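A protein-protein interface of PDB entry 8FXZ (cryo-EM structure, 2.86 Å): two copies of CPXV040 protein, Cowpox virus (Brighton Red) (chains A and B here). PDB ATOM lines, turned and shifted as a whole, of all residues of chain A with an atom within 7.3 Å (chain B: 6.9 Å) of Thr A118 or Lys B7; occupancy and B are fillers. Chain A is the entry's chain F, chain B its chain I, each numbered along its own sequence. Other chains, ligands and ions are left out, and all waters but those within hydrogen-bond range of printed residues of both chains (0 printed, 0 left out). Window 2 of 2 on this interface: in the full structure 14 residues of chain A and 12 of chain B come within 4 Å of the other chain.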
ATOM      1  N   ILE A 109      12.232  15.431  25.107  1.00  0.00           N
ATOM      2  CA  ILE A 109      11.764  14.152  24.583  1.00  0.00           C
ATOM      3  C   ILE A 109      12.010  13.093  25.640  1.00  0.00           C
ATOM      4  O   ILE A 109      13.151  12.895  26.071  1.00  0.00           O
ATOM      5  CB  ILE A 109      12.466  13.777  23.273  1.00  0.00           C
ATOM      6  CG1 ILE A 109      12.196  14.837  22.211  1.00  0.00           C
ATOM      7  CG2 ILE A 109      11.973  12.442  22.788  1.00  0.00           C
ATOM      8  CD1 ILE A 109      13.129  14.779  21.044  1.00  0.00           C
ATOM      9  N   ASN A 115      13.638   1.650  26.063  1.00  0.00           N
ATOM     10  CA  ASN A 115      14.897   2.334  26.336  1.00  0.00           C
ATOM     11  C   ASN A 115      14.698   3.568  27.214  1.00  0.00           C
ATOM     12  O   ASN A 115      15.241   4.639  26.956  1.00  0.00           O
ATOM     13  CB  ASN A 115      15.597   2.681  25.029  1.00  0.00           C
ATOM     14  CG  ASN A 115      16.133   1.459  24.327  1.00  0.00           C
ATOM     15  OD1 ASN A 115      17.303   1.114  24.472  1.00  0.00           O
ATOM     16  ND2 ASN A 115      15.279   0.789  23.571  1.00  0.00           N
ATOM     17  N   CYS A 116      13.936   3.397  28.284  1.00  0.00           N
ATOM     18  CA  CYS A 116      13.719   4.457  29.250  1.00  0.00           C
ATOM     19  C   CYS A 116      14.956   4.657  30.118  1.00  0.00           C
ATOM     20  O   CYS A 116      15.803   3.772  30.249  1.00  0.00           O
ATOM     21  CB  CYS A 116      12.516   4.134  30.122  1.00  0.00           C
ATOM     22  SG  CYS A 116      11.083   3.586  29.190  1.00  0.00           S
ATOM     23  N   GLY A 117      15.057   5.837  30.713  1.00  0.00           N
ATOM     24  CA  GLY A 117      16.224   6.159  31.506  1.00  0.00           C
ATOM     25  C   GLY A 117      16.090   7.513  32.158  1.00  0.00           C
ATOM     26  O   GLY A 117      14.988   8.039  32.312  1.00  0.00           O
ATOM     27  N   THR A 118      17.225   8.063  32.565  1.00  0.00           N
ATOM     28  CA  THR A 118      17.312   9.395  33.129  1.00  0.00           C
ATOM     29  C   THR A 118      17.710  10.371  32.020  1.00  0.00           C
ATOM     30  O   THR A 118      17.585  10.061  30.830  1.00  0.00           O
ATOM     31  CB  THR A 118      18.298   9.392  34.300  1.00  0.00           C
ATOM     32  OG1 THR A 118      19.595   9.007  33.839  1.00  0.00           O
ATOM     33  CG2 THR A 118      17.845   8.427  35.373  1.00  0.00           C
ATOM     34  N   THR A 119      18.186  11.556  32.394  1.00  0.00           N
ATOM     35  CA  THR A 119      18.481  12.596  31.415  1.00  0.00           C
ATOM     36  C   THR A 119      19.747  12.234  30.664  1.00  0.00           C
ATOM     37  O   THR A 119      20.855  12.470  31.141  1.00  0.00           O
ATOM     38  CB  THR A 119      18.621  13.947  32.095  1.00  0.00           C
ATOM     39  OG1 THR A 119      17.442  14.218  32.860  1.00  0.00           O
ATOM     40  CG2 THR A 119      18.796  15.028  31.063  1.00  0.00           C
ATOM     41  N   LYS A 120      19.583  11.677  29.467  1.00  0.00           N
ATOM     42  CA  LYS A 120      20.731  11.290  28.663  1.00  0.00           C
ATOM     43  C   LYS A 120      21.368  12.475  27.966  1.00  0.00           C
ATOM     44  O   LYS A 120      22.574  12.452  27.708  1.00  0.00           O
ATOM     45  CB  LYS A 120      20.329  10.258  27.619  1.00  0.00           C
ATOM     46  CG  LYS A 120      21.477   9.867  26.724  1.00  0.00           C
ATOM     47  CD  LYS A 120      21.228   8.562  26.020  1.00  0.00           C
ATOM     48  CE  LYS A 120      22.499   8.052  25.382  1.00  0.00           C
ATOM     49  NZ  LYS A 120      22.312   6.720  24.751  1.00  0.00           N
ATOM     50  N   TYR A 121      20.586  13.503  27.634  1.00  0.00           N
ATOM     51  CA  TYR A 121      21.135  14.655  26.928  1.00  0.00           C
ATOM     52  C   TYR A 121      20.490  15.939  27.424  1.00  0.00           C
ATOM     53  O   TYR A 121      19.299  15.959  27.740  1.00  0.00           O
ATOM     54  CB  TYR A 121      20.928  14.526  25.420  1.00  0.00           C
ATOM     55  CG  TYR A 121      21.747  15.482  24.599  1.00  0.00           C
ATOM     56  CD1 TYR A 121      23.125  15.380  24.549  1.00  0.00           C
ATOM     57  CD2 TYR A 121      21.142  16.472  23.854  1.00  0.00           C
ATOM     58  CE1 TYR A 121      23.871  16.247  23.795  1.00  0.00           C
ATOM     59  CE2 TYR A 121      21.879  17.339  23.101  1.00  0.00           C
ATOM     60  CZ  TYR A 121      23.243  17.223  23.075  1.00  0.00           C
ATOM     61  OH  TYR A 121      23.988  18.092  22.319  1.00  0.00           O
ATOM     62  N   ILE A 139      16.796  15.158  26.542  1.00  0.00           N
ATOM     63  CA  ILE A 139      16.405  13.812  26.143  1.00  0.00           C
ATOM     64  C   ILE A 139      16.546  12.901  27.349  1.00  0.00           C
ATOM     65  O   ILE A 139      17.659  12.724  27.870  1.00  0.00           O
ATOM     66  CB  ILE A 139      17.246  13.297  24.967  1.00  0.00           C
ATOM     67  CG1 ILE A 139      16.934  14.121  23.720  1.00  0.00           C
ATOM     68  CG2 ILE A 139      16.970  11.827  24.730  1.00  0.00           C
ATOM     69  CD1 ILE A 139      17.778  13.784  22.536  1.00  0.00           C
ATOM     70  N   ASN A 140      15.413  12.336  27.790  1.00  0.00           N
ATOM     71  CA  ASN A 140      15.298  11.403  28.909  1.00  0.00           C
ATOM     72  C   ASN A 140      15.044  10.013  28.334  1.00  0.00           C
ATOM     73  O   ASN A 140      13.897   9.639  28.057  1.00  0.00           O
ATOM     74  CB  ASN A 140      14.164  11.809  29.843  1.00  0.00           C
ATOM     75  CG  ASN A 140      14.611  12.732  30.941  1.00  0.00           C
ATOM     76  OD1 ASN A 140      15.471  13.584  30.738  1.00  0.00           O
ATOM     77  ND2 ASN A 140      14.032  12.568  32.125  1.00  0.00           N
ATOM     78  N   GLY A 141      16.119   9.251  28.165  1.00  0.00           N
ATOM     79  CA  GLY A 141      16.049   7.914  27.618  1.00  0.00           C
ATOM     80  C   GLY A 141      17.207   7.634  26.687  1.00  0.00           C
ATOM     81  O   GLY A 141      18.033   8.516  26.452  1.00  0.00           O
ATOM     82  N   SER A 142      17.285   6.425  26.150  1.00  0.00           N
ATOM     83  CA  SER A 142      18.304   6.048  25.182  1.00  0.00           C
ATOM     84  C   SER A 142      17.655   5.529  23.910  1.00  0.00           C
ATOM     85  O   SER A 142      18.071   4.518  23.343  1.00  0.00           O
ATOM     86  CB  SER A 142      19.251   5.005  25.764  1.00  0.00           C
ATOM     87  OG  SER A 142      18.542   3.864  26.206  1.00  0.00           O
ATOM     88  N   ALA B   4      24.851  12.541  38.031  1.00  0.00           N
ATOM     89  CA  ALA B   4      24.197  12.790  36.752  1.00  0.00           C
ATOM     90  C   ALA B   4      24.769  11.880  35.669  1.00  0.00           C
ATOM     91  O   ALA B   4      25.037  12.322  34.552  1.00  0.00           O
ATOM     92  CB  ALA B   4      24.351  14.249  36.353  1.00  0.00           C
ATOM     93  N   GLU B   5      24.952  10.607  36.009  1.00  0.00           N
ATOM     94  CA  GLU B   5      25.479   9.612  35.083  1.00  0.00           C
ATOM     95  C   GLU B   5      24.337   8.715  34.621  1.00  0.00           C
ATOM     96  O   GLU B   5      23.567   8.210  35.444  1.00  0.00           O
ATOM     97  CB  GLU B   5      26.581   8.785  35.746  1.00  0.00           C
ATOM     98  CG  GLU B   5      27.677   8.335  34.792  1.00  0.00           C
ATOM     99  CD  GLU B   5      27.187   7.339  33.761  1.00  0.00           C
ATOM    100  OE1 GLU B   5      26.281   6.545  34.085  1.00  0.00           O
ATOM    101  OE2 GLU B   5      27.708   7.351  32.626  1.00  0.00           O
ATOM    102  N   TYR B   6      24.234   8.521  33.309  1.00  0.00           N
ATOM    103  CA  TYR B   6      23.080   7.837  32.746  1.00  0.00           C
ATOM    104  C   TYR B   6      23.065   6.365  33.136  1.00  0.00           C
ATOM    105  O   TYR B   6      24.090   5.680  33.094  1.00  0.00           O
ATOM    106  CB  TYR B   6      23.079   7.969  31.225  1.00  0.00           C
ATOM    107  CG  TYR B   6      21.898   7.308  30.566  1.00  0.00           C
ATOM    108  CD1 TYR B   6      20.611   7.715  30.849  1.00  0.00           C
ATOM    109  CD2 TYR B   6      22.071   6.282  29.661  1.00  0.00           C
ATOM    110  CE1 TYR B   6      19.533   7.114  30.259  1.00  0.00           C
ATOM    111  CE2 TYR B   6      21.000   5.682  29.063  1.00  0.00           C
ATOM    112  CZ  TYR B   6      19.732   6.100  29.367  1.00  0.00           C
ATOM    113  OH  TYR B   6      18.650   5.500  28.769  1.00  0.00           O
ATOM    114  N   LYS B   7      21.884   5.877  33.511  1.00  0.00           N
ATOM    115  CA  LYS B   7      21.666   4.457  33.748  1.00  0.00           C
ATOM    116  C   LYS B   7      20.257   4.110  33.297  1.00  0.00           C
ATOM    117  O   LYS B   7      19.315   4.842  33.605  1.00  0.00           O
ATOM    118  CB  LYS B   7      21.858   4.106  35.226  1.00  0.00           C
ATOM    119  CG  LYS B   7      20.898   4.821  36.166  1.00  0.00           C
ATOM    120  CD  LYS B   7      21.186   4.485  37.621  1.00  0.00           C
ATOM    121  CE  LYS B   7      20.188   5.153  38.552  1.00  0.00           C
ATOM    122  NZ  LYS B   7      20.229   6.638  38.446  1.00  0.00           N
ATOM    123  N   ASN B   8      20.116   3.001  32.577  1.00  0.00           N
ATOM    124  CA  ASN B   8      18.804   2.587  32.098  1.00  0.00           C
ATOM    125  C   ASN B   8      17.889   2.253  33.266  1.00  0.00           C
ATOM    126  O   ASN B   8      18.336   1.832  34.334  1.00  0.00           O
ATOM    127  CB  ASN B   8      18.922   1.376  31.182  1.00  0.00           C
ATOM    128  CG  ASN B   8      19.384   1.735  29.795  1.00  0.00           C
ATOM    129  OD1 ASN B   8      20.580   1.813  29.532  1.00  0.00           O
ATOM    130  ND2 ASN B   8      18.439   1.941  28.893  1.00  0.00           N
ATOM    131  N   THR B   9      16.595   2.458  33.060  1.00  0.00           N
ATOM    132  CA  THR B   9      15.611   2.198  34.092  1.00  0.00           C
ATOM    133  C   THR B   9      14.411   1.506  33.470  1.00  0.00           C
ATOM    134  O   THR B   9      14.155   1.614  32.271  1.00  0.00           O
ATOM    135  CB  THR B   9      15.165   3.486  34.797  1.00  0.00           C
ATOM    136  OG1 THR B   9      14.275   4.218  33.949  1.00  0.00           O
ATOM    137  CG2 THR B   9      16.357   4.353  35.138  1.00  0.00           C
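The side-chain amide nitrogen (ND2) of Asn B8 is in hydrogen-bond range of the backbone carbonyl oxygen (O) of Cys A116 (3.5 Å).
The backbone carbonyl oxygen of Cys A116 sits at hydrogen-bond distance from the backbone NH of Thr B9 (3.2 Å).
OG of Ser A142 sits at hydrogen-bond distance from OH of Tyr B6 (3.0 Å).
The side-chain amide nitrogen (ND2) of Asn B8 lies within hydrogen-bond range of the side-chain hydroxyl (OG) of Ser A142, 3.3 Å away.
The backbone carbonyl oxygen (O) of Asn A115 is in hydrogen-bond range of the backbone NH (N) of Ser A142.
The backbone carbonyl oxygen (O) of Thr A118 lies within hydrogen-bond range of the backbone NH (N) of Gly A141, 3.1 Å away.
Among the printed residues, merely in contact across the chains: Asn A115 with Tyr B6 (3.96 Å), Cys A116 with Tyr B6 (3.6 Å), Gly A117 with Tyr B6 (3.7 Å), Gly A117 with Lys B7 (3.96 Å), Gly A117 with Thr B9 (3.7 Å), Thr A118 with Tyr B6 (3.4 Å), Thr A118 with Lys B7 (3.9 Å) and Gly A141 with Tyr B6 (3.3 Å).
Printed residues of chain B within 4 Å of Asn A115: Tyr B6 (3.96 Å).
Of the printed residues of chain B, Cys A116 touches Tyr B6 (3.6 Å), Asn B8 (3.5 Å) and Thr B9 (3.2 Å).
Thr A118 touches just these residues of chain B: Tyr B6 and Lys B7.
Ile A139 touches none of the printed residues of chain B.
Of the printed residues of chain B, Gly A141 touches Tyr B6.
Printed residues of chain B within 4 Å of Ser A142: Tyr B6 and Asn B8.
Of the printed residues of chain A, Tyr B6 touches Asn A115 (3.96 Å), Cys A116 (3.6 Å), Gly A117 (3.7 Å), Thr A118 (3.4 Å), Gly A141 (3.3 Å) and Ser A142 (3.0 Å).
Lys B7 touches just these residues of chain A: Gly A117 (3.96 Å) and Thr A118 (3.9 Å).
The nearest residue of chain A that does not touch Lys B7 is Cys A116 (5.0 Å).
The nearest printed residue of chain A that does not touch Asn B8 is Asn A115 (4.4 Å).
Of the 12 printed residues of chain A, 6 touch a printed residue of chain B.
Printed residues of chain A that touch a printed residue of chain B: Asn A115, Cys A116, Gly A117, Thr A118, Gly A141 and Ser A142.
Of the 6 printed residues of chain B, 4 touch a printed residue of chain A.
Hydrophobic or aromatic side chains of chain B that line the printed part of chain A: Tyr B6.
Among the printed residues, 12 pairs touch across the chains.
Among the printed residues, no Asp or Glu carboxylate lies within 4 Å of a Lys or Arg side-chain nitrogen of the other chain.
No position is printed for both chains.
Of the 12 pairs that touch across the chains among the printed residues, none has its exchanged pair printed and touching as well.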
